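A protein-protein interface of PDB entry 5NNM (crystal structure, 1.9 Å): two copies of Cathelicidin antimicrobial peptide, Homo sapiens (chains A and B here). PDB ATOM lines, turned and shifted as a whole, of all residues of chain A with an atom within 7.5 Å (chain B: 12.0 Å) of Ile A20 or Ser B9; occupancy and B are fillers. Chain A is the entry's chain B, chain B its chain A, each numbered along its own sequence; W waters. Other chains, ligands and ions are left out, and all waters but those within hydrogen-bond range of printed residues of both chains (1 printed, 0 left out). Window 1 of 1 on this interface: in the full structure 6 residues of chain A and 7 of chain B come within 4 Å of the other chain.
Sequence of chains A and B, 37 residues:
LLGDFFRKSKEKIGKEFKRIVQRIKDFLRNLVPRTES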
ATOM      1  N   LYS A  15       1.409   1.306   8.971  1.00  0.00           N
ATOM      2  CA  LYS A  15       2.391   1.638  10.061  1.00  0.00           C
ATOM      3  C   LYS A  15       1.778   2.185  11.421  1.00  0.00           C
ATOM      4  O   LYS A  15       2.295   1.875  12.519  1.00  0.00           O
ATOM      5  CB  LYS A  15       3.408   2.688   9.581  1.00  0.00           C
ATOM      6  CG  LYS A  15       4.920   2.355   9.720  1.00  0.00           C
ATOM      7  CD  LYS A  15       5.668   2.156   8.396  1.00  0.00           C
ATOM      8  CE  LYS A  15       5.614   0.728   7.921  1.00  0.00           C
ATOM      9  NZ  LYS A  15       5.563   0.639   6.436  1.00  0.00           N
ATOM     10  N   GLU A  16       0.728   3.005  11.351  1.00  0.00           N
ATOM     11  CA  GLU A  16      -0.029   3.410  12.583  1.00  0.00           C
ATOM     12  C   GLU A  16      -0.955   2.350  13.275  1.00  0.00           C
ATOM     13  O   GLU A  16      -0.964   2.327  14.544  1.00  0.00           O
ATOM     14  CB  GLU A  16      -0.779   4.753  12.405  1.00  0.00           C
ATOM     15  CG  GLU A  16       0.125   5.939  12.813  1.00  0.00           C
ATOM     16  CD  GLU A  16      -0.021   6.692  14.190  1.00  0.00           C
ATOM     17  OE1 GLU A  16       0.573   7.781  14.154  1.00  0.00           O
ATOM     18  OE2 GLU A  16      -0.538   6.305  15.295  1.00  0.00           O
ATOM     19  N   PHE A  17      -1.716   1.516  12.509  1.00  0.00           N
ATOM     20  CA  PHE A  17      -2.469   0.313  13.038  1.00  0.00           C
ATOM     21  C   PHE A  17      -1.468  -0.640  13.808  1.00  0.00           C
ATOM     22  O   PHE A  17      -1.856  -1.199  14.838  1.00  0.00           O
ATOM     23  CB  PHE A  17      -3.368  -0.467  11.957  1.00  0.00           C
ATOM     24  CG  PHE A  17      -4.836   0.069  11.719  1.00  0.00           C
ATOM     25  CD1 PHE A  17      -5.867  -0.083  12.668  1.00  0.00           C
ATOM     26  CD2 PHE A  17      -5.193   0.686  10.511  1.00  0.00           C
ATOM     27  CE1 PHE A  17      -7.156   0.431  12.437  1.00  0.00           C
ATOM     28  CE2 PHE A  17      -6.494   1.162  10.278  1.00  0.00           C
ATOM     29  CZ  PHE A  17      -7.484   1.038  11.223  1.00  0.00           C
ATOM     30  N   LYS A  18      -0.197  -0.773  13.387  1.00  0.00           N
ATOM     31  CA  LYS A  18       0.844  -1.593  14.117  1.00  0.00           C
ATOM     32  C   LYS A  18       1.398  -1.035  15.472  1.00  0.00           C
ATOM     33  O   LYS A  18       1.745  -1.857  16.359  1.00  0.00           O
ATOM     34  CB  LYS A  18       2.051  -1.993  13.201  1.00  0.00           C
ATOM     35  CG  LYS A  18       1.752  -3.006  12.070  1.00  0.00           C
ATOM     36  CD  LYS A  18       3.001  -3.302  11.197  1.00  0.00           C
ATOM     37  CE  LYS A  18       2.819  -3.219   9.672  1.00  0.00           C
ATOM     38  NZ  LYS A  18       3.400  -2.006   9.002  1.00  0.00           N
ATOM     39  N   ARG A  19       1.515   0.297  15.610  1.00  0.00           N
ATOM     40  CA  ARG A  19       1.850   0.968  16.897  1.00  0.00           C
ATOM     41  C   ARG A  19       0.747   0.777  18.017  1.00  0.00           C
ATOM     42  O   ARG A  19       1.083   0.590  19.227  1.00  0.00           O
ATOM     43  CB  ARG A  19       2.201   2.476  16.641  1.00  0.00           C
ATOM     44  CG  ARG A  19       3.548   2.745  15.919  1.00  0.00           C
ATOM     45  CD  ARG A  19       3.857   4.235  15.689  1.00  0.00           C
ATOM     46  NE  ARG A  19       4.909   4.422  14.652  1.00  0.00           N
ATOM     47  CZ  ARG A  19       4.742   4.921  13.414  1.00  0.00           C
ATOM     48  NH1 ARG A  19       3.565   5.349  12.962  1.00  0.00           N
ATOM     49  NH2 ARG A  19       5.797   5.000  12.607  1.00  0.00           N
ATOM     50  N   ILE A  20      -0.559   0.832  17.655  1.00  0.00           N
ATOM     51  CA  ILE A  20      -1.747   0.463  18.526  1.00  0.00           C
ATOM     52  C   ILE A  20      -1.728  -1.029  19.118  1.00  0.00           C
ATOM     53  O   ILE A  20      -1.938  -1.232  20.359  1.00  0.00           O
ATOM     54  CB  ILE A  20      -3.104   0.791  17.825  1.00  0.00           C
ATOM     55  CG1 ILE A  20      -3.277   2.330  17.540  1.00  0.00           C
ATOM     56  CG2 ILE A  20      -4.340   0.355  18.606  1.00  0.00           C
ATOM     57  CD1 ILE A  20      -4.482   2.707  16.690  1.00  0.00           C
ATOM     58  N   VAL A  21      -1.467  -2.041  18.257  1.00  0.00           N
ATOM     59  CA  VAL A  21      -1.260  -3.450  18.687  1.00  0.00           C
ATOM     60  C   VAL A  21      -0.112  -3.685  19.759  1.00  0.00           C
ATOM     61  O   VAL A  21      -0.353  -4.368  20.802  1.00  0.00           O
ATOM     62  CB  VAL A  21      -1.150  -4.425  17.449  1.00  0.00           C
ATOM     63  CG1 VAL A  21      -0.784  -5.875  17.882  1.00  0.00           C
ATOM     64  CG2 VAL A  21      -2.473  -4.445  16.628  1.00  0.00           C
ATOM     65  N   GLN A  22       1.078  -3.115  19.572  1.00  0.00           N
ATOM     66  CA  GLN A  22       2.139  -3.163  20.588  1.00  0.00           C
ATOM     67  C   GLN A  22       1.909  -2.432  21.949  1.00  0.00           C
ATOM     68  O   GLN A  22       2.361  -2.971  23.030  1.00  0.00           O
ATOM     69  CB  GLN A  22       3.479  -2.735  20.013  1.00  0.00           C
ATOM     70  CG  GLN A  22       4.031  -3.755  18.990  1.00  0.00           C
ATOM     71  CD  GLN A  22       4.172  -5.210  19.450  1.00  0.00           C
ATOM     72  OE1 GLN A  22       4.427  -5.467  20.626  1.00  0.00           O
ATOM     73  NE2 GLN A  22       4.094  -6.171  18.493  1.00  0.00           N
ATOM     74  N   ARG A  23       1.253  -1.273  21.947  1.00  0.00           N
ATOM     75  CA  ARG A  23       0.848  -0.608  23.238  1.00  0.00           C
ATOM     76  C   ARG A  23      -0.138  -1.460  24.155  1.00  0.00           C
ATOM     77  O   ARG A  23       0.076  -1.490  25.410  1.00  0.00           O
ATOM     78  CB  ARG A  23       0.359   0.862  23.014  1.00  0.00           C
ATOM     79  CG  ARG A  23       0.198   1.790  24.289  1.00  0.00           C
ATOM     80  CD  ARG A  23       1.498   2.090  25.152  1.00  0.00           C
ATOM     81  NE  ARG A  23       1.272   2.785  26.477  1.00  0.00           N
ATOM     82  CZ  ARG A  23       1.410   4.111  26.743  1.00  0.00           C
ATOM     83  NH1 ARG A  23       1.828   4.972  25.811  1.00  0.00           N
ATOM     84  NH2 ARG A  23       1.126   4.601  27.973  1.00  0.00           N
ATOM     85  N   ILE A  24      -1.137  -2.143  23.537  1.00  0.00           N
ATOM     86  CA  ILE A  24      -2.106  -3.094  24.222  1.00  0.00           C
ATOM     87  C   ILE A  24      -1.327  -4.307  24.911  1.00  0.00           C
ATOM     88  O   ILE A  24      -1.608  -4.668  26.104  1.00  0.00           O
ATOM     89  CB  ILE A  24      -3.348  -3.527  23.265  1.00  0.00           C
ATOM     90  CG1 ILE A  24      -4.257  -2.345  22.811  1.00  0.00           C
ATOM     91  CG2 ILE A  24      -4.247  -4.631  23.896  1.00  0.00           C
ATOM     92  CD1 ILE A  24      -5.294  -2.619  21.677  1.00  0.00           C
ATOM     93  N   LYS A  25      -0.321  -4.860  24.217  1.00  0.00           N
ATOM     94  CA  LYS A  25       0.511  -5.972  24.753  1.00  0.00           C
ATOM     95  C   LYS A  25       1.397  -5.613  25.988  1.00  0.00           C
ATOM     96  O   LYS A  25       1.611  -6.464  26.899  1.00  0.00           O
ATOM     97  CB  LYS A  25       1.355  -6.634  23.619  1.00  0.00           C
ATOM     98  CG  LYS A  25       0.556  -7.550  22.649  1.00  0.00           C
ATOM     99  CD  LYS A  25       1.418  -8.233  21.561  1.00  0.00           C
ATOM    100  CE  LYS A  25       0.704  -9.372  20.816  1.00  0.00           C
ATOM    101  NZ  LYS A  25       1.227  -9.549  19.426  1.00  0.00           N
ATOM    102  N   LEU B   1      -0.456   9.035  30.724  1.00  0.00           N
ATOM    103  CA  LEU B   1      -1.129   9.525  29.507  1.00  0.00           C
ATOM    104  C   LEU B   1      -1.925   8.444  28.744  1.00  0.00           C
ATOM    105  O   LEU B   1      -2.199   8.716  27.592  1.00  0.00           O
ATOM    106  CB  LEU B   1      -0.096  10.211  28.559  1.00  0.00           C
ATOM    107  CG  LEU B   1       0.775   9.538  27.430  1.00  0.00           C
ATOM    108  CD1 LEU B   1       0.930   8.065  27.618  1.00  0.00           C
ATOM    109  CD2 LEU B   1       0.180   9.872  26.109  1.00  0.00           C
ATOM    110  N   LEU B   2      -2.349   7.284  29.312  1.00  0.00           N
ATOM    111  CA  LEU B   2      -3.002   6.215  28.393  1.00  0.00           C
ATOM    112  C   LEU B   2      -4.278   6.606  27.572  1.00  0.00           C
ATOM    113  O   LEU B   2      -4.337   6.247  26.354  1.00  0.00           O
ATOM    114  CB  LEU B   2      -3.222   4.803  29.075  1.00  0.00           C
ATOM    115  CG  LEU B   2      -3.459   3.542  28.173  1.00  0.00           C
ATOM    116  CD1 LEU B   2      -2.200   3.218  27.326  1.00  0.00           C
ATOM    117  CD2 LEU B   2      -3.892   2.257  28.903  1.00  0.00           C
ATOM    118  N   GLY B   3      -5.234   7.323  28.198  1.00  0.00           N
ATOM    119  CA  GLY B   3      -6.382   7.889  27.525  1.00  0.00           C
ATOM    120  C   GLY B   3      -6.066   8.993  26.468  1.00  0.00           C
ATOM    121  O   GLY B   3      -6.828   9.082  25.421  1.00  0.00           O
ATOM    122  N   ASP B   4      -5.029   9.850  26.750  1.00  0.00           N
ATOM    123  CA  ASP B   4      -4.447  10.873  25.769  1.00  0.00           C
ATOM    124  C   ASP B   4      -3.812  10.109  24.484  1.00  0.00           C
ATOM    125  O   ASP B   4      -4.022  10.588  23.333  1.00  0.00           O
ATOM    126  CB  ASP B   4      -3.374  11.839  26.380  1.00  0.00           C
ATOM    127  CG  ASP B   4      -3.882  12.667  27.693  1.00  0.00           C
ATOM    128  OD1 ASP B   4      -4.795  13.526  27.660  1.00  0.00           O
ATOM    129  OD2 ASP B   4      -3.328  12.397  28.809  1.00  0.00           O
ATOM    130  N   PHE B   5      -3.088   8.955  24.677  1.00  0.00           N
ATOM    131  CA  PHE B   5      -2.593   8.062  23.505  1.00  0.00           C
ATOM    132  C   PHE B   5      -3.692   7.552  22.523  1.00  0.00           C
ATOM    133  O   PHE B   5      -3.590   7.827  21.280  1.00  0.00           O
ATOM    134  CB  PHE B   5      -1.664   6.919  23.958  1.00  0.00           C
ATOM    135  CG  PHE B   5      -1.212   5.972  22.809  1.00  0.00           C
ATOM    136  CD1 PHE B   5      -0.154   6.279  21.987  1.00  0.00           C
ATOM    137  CD2 PHE B   5      -1.880   4.768  22.580  1.00  0.00           C
ATOM    138  CE1 PHE B   5       0.215   5.413  20.909  1.00  0.00           C
ATOM    139  CE2 PHE B   5      -1.515   3.901  21.548  1.00  0.00           C
ATOM    140  CZ  PHE B   5      -0.466   4.216  20.710  1.00  0.00           C
ATOM    141  N   PHE B   6      -4.762   6.913  23.048  1.00  0.00           N
ATOM    142  CA  PHE B   6      -5.910   6.453  22.219  1.00  0.00           C
ATOM    143  C   PHE B   6      -6.692   7.610  21.414  1.00  0.00           C
ATOM    144  O   PHE B   6      -7.035   7.404  20.217  1.00  0.00           O
ATOM    145  CB  PHE B   6      -6.906   5.496  23.006  1.00  0.00           C
ATOM    146  CG  PHE B   6      -6.322   4.096  23.486  1.00  0.00           C
ATOM    147  CD1 PHE B   6      -5.610   3.203  22.624  1.00  0.00           C
ATOM    148  CD2 PHE B   6      -6.598   3.615  24.824  1.00  0.00           C
ATOM    149  CE1 PHE B   6      -5.128   1.948  23.104  1.00  0.00           C
ATOM    150  CE2 PHE B   6      -6.084   2.352  25.309  1.00  0.00           C
ATOM    151  CZ  PHE B   6      -5.340   1.520  24.457  1.00  0.00           C
ATOM    152  N   ARG B   7      -7.018   8.772  22.033  1.00  0.00           N
ATOM    153  CA  ARG B   7      -7.671  10.010  21.362  1.00  0.00           C
ATOM    154  C   ARG B   7      -6.885  10.636  20.137  1.00  0.00           C
ATOM    155  O   ARG B   7      -7.548  10.964  19.086  1.00  0.00           O
ATOM    156  CB  ARG B   7      -7.967  11.155  22.421  1.00  0.00           C
ATOM    157  CG  ARG B   7      -8.870  12.317  21.960  1.00  0.00           C
ATOM    158  CD  ARG B   7      -8.595  13.733  22.575  1.00  0.00           C
ATOM    159  NE  ARG B   7      -8.208  13.697  23.969  1.00  0.00           N
ATOM    160  CZ  ARG B   7      -7.090  14.186  24.539  1.00  0.00           C
ATOM    161  NH1 ARG B   7      -6.191  14.895  23.873  1.00  0.00           N
ATOM    162  NH2 ARG B   7      -6.878  13.978  25.846  1.00  0.00           N
ATOM    163  N   LYS B   8      -5.528  10.793  20.269  1.00  0.00           N
ATOM    164  CA  LYS B   8      -4.655  11.410  19.276  1.00  0.00           C
ATOM    165  C   LYS B   8      -4.294  10.442  18.039  1.00  0.00           C
ATOM    166  O   LYS B   8      -4.015  10.947  16.907  1.00  0.00           O
ATOM    167  CB  LYS B   8      -3.360  11.992  19.932  1.00  0.00           C
ATOM    168  CG  LYS B   8      -3.557  13.244  20.811  1.00  0.00           C
ATOM    169  CD  LYS B   8      -2.295  13.627  21.607  1.00  0.00           C
ATOM    170  CE  LYS B   8      -2.175  15.156  21.863  1.00  0.00           C
ATOM    171  NZ  LYS B   8      -0.788  15.678  22.127  1.00  0.00           N
ATOM    172  N   SER B   9      -4.284   9.113  18.265  1.00  0.00           N
ATOM    173  CA  SER B   9      -4.060   8.062  17.211  1.00  0.00           C
ATOM    174  C   SER B   9      -5.261   7.917  16.190  1.00  0.00           C
ATOM    175  O   SER B   9      -5.043   7.779  14.948  1.00  0.00           O
ATOM    176  CB  SER B   9      -3.610   6.725  17.869  1.00  0.00           C
ATOM    177  OG  SER B   9      -4.655   5.967  18.476  1.00  0.00           O
ATOM    178  N   LYS B  10      -6.504   7.994  16.686  1.00  0.00           N
ATOM    179  CA  LYS B  10      -7.754   8.123  15.857  1.00  0.00           C
ATOM    180  C   LYS B  10      -7.861   9.401  14.950  1.00  0.00           C
ATOM    181  O   LYS B  10      -8.255   9.266  13.749  1.00  0.00           O
ATOM    182  CB  LYS B  10      -9.014   7.964  16.735  1.00  0.00           C
ATOM    183  CG  LYS B  10     -10.373   8.361  16.113  1.00  0.00           C
ATOM    184  CD  LYS B  10     -11.573   8.663  17.062  1.00  0.00           C
ATOM    185  CE  LYS B  10     -11.992   7.411  17.872  1.00  0.00           C
ATOM    186  NZ  LYS B  10     -13.008   6.560  17.164  1.00  0.00           N
ATOM    187  N   GLU B  11      -7.527  10.609  15.498  1.00  0.00           N
ATOM    188  CA  GLU B  11      -7.380  11.941  14.735  1.00  0.00           C
ATOM    189  C   GLU B  11      -6.403  11.911  13.462  1.00  0.00           C
ATOM    190  O   GLU B  11      -6.695  12.463  12.394  1.00  0.00           O
ATOM    191  CB  GLU B  11      -6.871  13.067  15.679  1.00  0.00           C
ATOM    192  CG  GLU B  11      -7.899  13.811  16.557  1.00  0.00           C
ATOM    193  CD  GLU B  11      -7.253  14.822  17.581  1.00  0.00           C
ATOM    194  OE1 GLU B  11      -7.870  15.105  18.667  1.00  0.00           O
ATOM    195  OE2 GLU B  11      -6.124  15.336  17.308  1.00  0.00           O
ATOM    196  N   LYS B  12      -5.241  11.314  13.657  1.00  0.00           N
ATOM    197  CA  LYS B  12      -4.199  11.097  12.657  1.00  0.00           C
ATOM    198  C   LYS B  12      -4.618  10.174  11.369  1.00  0.00           C
ATOM    199  O   LYS B  12      -4.377  10.584  10.157  1.00  0.00           O
ATOM    200  CB  LYS B  12      -3.072  10.537  13.509  1.00  0.00           C
ATOM    201  CG  LYS B  12      -1.635  10.864  13.212  1.00  0.00           C
ATOM    202  CD  LYS B  12      -0.842  11.308  14.478  1.00  0.00           C
ATOM    203  CE  LYS B  12      -0.656  10.227  15.572  1.00  0.00           C
ATOM    204  NZ  LYS B  12       0.772   9.874  15.914  1.00  0.00           N
ATOM    205  N   ILE B  13      -5.265   8.998  11.635  1.00  0.00           N
ATOM    206  CA  ILE B  13      -5.954   8.099  10.627  1.00  0.00           C
ATOM    207  C   ILE B  13      -7.137   8.777   9.840  1.00  0.00           C
ATOM    208  O   ILE B  13      -7.155   8.700   8.565  1.00  0.00           O
ATOM    209  CB  ILE B  13      -6.329   6.647  11.225  1.00  0.00           C
ATOM    210  CG1 ILE B  13      -5.058   5.841  11.604  1.00  0.00           C
ATOM    211  CG2 ILE B  13      -7.194   5.827  10.236  1.00  0.00           C
ATOM    212  CD1 ILE B  13      -5.248   4.537  12.410  1.00  0.00           C
ATOM    213  N   GLY B  14      -8.083   9.455  10.495  1.00  0.00           N
ATOM    214  CA  GLY B  14      -9.042  10.306   9.796  1.00  0.00           C
ATOM    215  C   GLY B  14      -8.559  11.449   8.852  1.00  0.00           C
ATOM    216  O   GLY B  14      -9.175  11.680   7.797  1.00  0.00           O
ATOM    217  N   LYS B  15      -7.495  12.159   9.208  1.00  0.00           N
ATOM    218  CA  LYS B  15      -6.813  13.174   8.320  1.00  0.00           C
ATOM    219  C   LYS B  15      -6.193  12.637   6.958  1.00  0.00           C
ATOM    220  O   LYS B  15      -6.205  13.341   5.914  1.00  0.00           O
ATOM    221  CB  LYS B  15      -5.706  13.920   9.129  1.00  0.00           C
ATOM    222  CG  LYS B  15      -6.194  15.129   9.926  1.00  0.00           C
ATOM    223  CD  LYS B  15      -5.127  16.190  10.213  1.00  0.00           C
ATOM    224  CE  LYS B  15      -4.224  15.848  11.429  1.00  0.00           C
ATOM    225  NZ  LYS B  15      -4.868  16.071  12.776  1.00  0.00           N
ATOM    226  N   GLU B  16      -5.611  11.458   6.999  1.00  0.00           N
ATOM    227  CA  GLU B  16      -5.121  10.769   5.745  1.00  0.00           C
ATOM    228  C   GLU B  16      -6.218  10.238   4.759  1.00  0.00           C
ATOM    229  O   GLU B  16      -6.028  10.401   3.492  1.00  0.00           O
ATOM    230  CB  GLU B  16      -4.038   9.681   6.005  1.00  0.00           C
ATOM    231  CG  GLU B  16      -2.545  10.058   5.944  1.00  0.00           C
ATOM    232  CD  GLU B  16      -1.959  10.593   4.581  1.00  0.00           C
ATOM    233  OE1 GLU B  16      -1.423  11.714   4.649  1.00  0.00           O
ATOM    234  OE2 GLU B  16      -1.959   9.945   3.468  1.00  0.00           O
ATOM    235  N   PHE B  17      -7.323   9.637   5.257  1.00  0.00           N
ATOM    236  CA  PHE B  17      -8.565   9.294   4.397  1.00  0.00           C
ATOM    237  C   PHE B  17      -9.126  10.555   3.654  1.00  0.00           C
ATOM    238  O   PHE B  17      -9.544  10.448   2.471  1.00  0.00           O
ATOM    239  CB  PHE B  17      -9.647   8.463   5.163  1.00  0.00           C
ATOM    240  CG  PHE B  17      -9.356   6.910   5.260  1.00  0.00           C
ATOM    241  CD1 PHE B  17      -9.523   6.064   4.140  1.00  0.00           C
ATOM    242  CD2 PHE B  17      -9.003   6.272   6.495  1.00  0.00           C
ATOM    243  CE1 PHE B  17      -9.273   4.673   4.236  1.00  0.00           C
ATOM    244  CE2 PHE B  17      -8.787   4.861   6.610  1.00  0.00           C
ATOM    245  CZ  PHE B  17      -8.905   4.062   5.465  1.00  0.00           C
ATOM    246  N   ARG B  19      -7.252  13.435   2.571  1.00  0.00           N
ATOM    247  CA  ARG B  19      -6.261  13.748   1.487  1.00  0.00           C
ATOM    248  C   ARG B  19      -6.464  12.881   0.134  1.00  0.00           C
ATOM    249  O   ARG B  19      -6.378  13.454  -1.008  1.00  0.00           O
ATOM    250  CB  ARG B  19      -4.796  13.684   2.015  1.00  0.00           C
ATOM    251  CG  ARG B  19      -4.366  14.835   2.997  1.00  0.00           C
ATOM    252  CD  ARG B  19      -2.873  14.703   3.422  1.00  0.00           C
ATOM    253  NE  ARG B  19      -2.330  15.498   4.566  1.00  0.00           N
ATOM    254  CZ  ARG B  19      -1.966  15.037   5.796  1.00  0.00           C
ATOM    255  NH1 ARG B  19      -2.127  13.764   6.173  1.00  0.00           N
ATOM    256  NH2 ARG B  19      -1.470  15.890   6.694  1.00  0.00           N
HETATM  257  O   HOH W   1       0.859   8.051  17.960  1.00  0.00           O
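Positions printed for both chains: 15, 16, 17 and 19.
Among the printed residues, merely in contact across the chains: Ile A20 with Ser B9, Arg A23 with Leu B1, Arg A23 with Leu B2 and Arg A23 with Phe B5.
No residue of chain B comes within 4 Å of Phe A17. Printed residues of chain B within 4 Å of Ile A20: Ser B9. No residue of chain B comes within 4 Å of Val A21. No residue of chain B comes within 4 Å of Gln A22. Of the printed residues of chain B, Arg A23 touches Leu B1, Leu B2 and Phe B5. No residue of chain B comes within 4 Å of Ile A24. Printed residues of chain A within 4 Å of Phe B5: Arg A23. Arg B7 touches none of the printed residues of chain A. Of the printed residues of chain A, Ser B9 touches Ile A20. Ile B13 touches none of the printed residues of chain A. The nearest printed residue of chain B that does not touch Ile A20 is Phe B5 (4.5 Å).
Printed residues of chain A that touch a printed residue of chain B: Glu A16, Ile A20 and Arg A23. Hydrophobic or aromatic side chains of chain A within 4 Å of the printed part of chain B: Ile A20. Printed residues of chain B that touch a printed residue of chain A: Leu B1, Leu B2, Phe B5, Ser B9 and Lys B12. Hydrophobic or aromatic side chains of chain B within 4 Å of the printed part of chain A: Leu B1, Leu B2 and Phe B5. Among the printed residues, Asp or Glu carboxylates within 4 Å of a Lys or Arg side-chain nitrogen of the other chain: Glu A16 with Lys B12.
The side-chain amino group (NZ) of Lys B12 lies within salt-bridge range of the side-chain carboxylate (OE1) of Glu A16 (2.7 Å).
O of Phe B6 lies within hydrogen-bond range of OG of Ser B9, 3.3 Å away.
Water W1 lies within hydrogen-bond range of the side-chain amino group of Lys B12 (2.7 Å) and the side-chain carboxylate of Glu A16 (3.5 Å).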
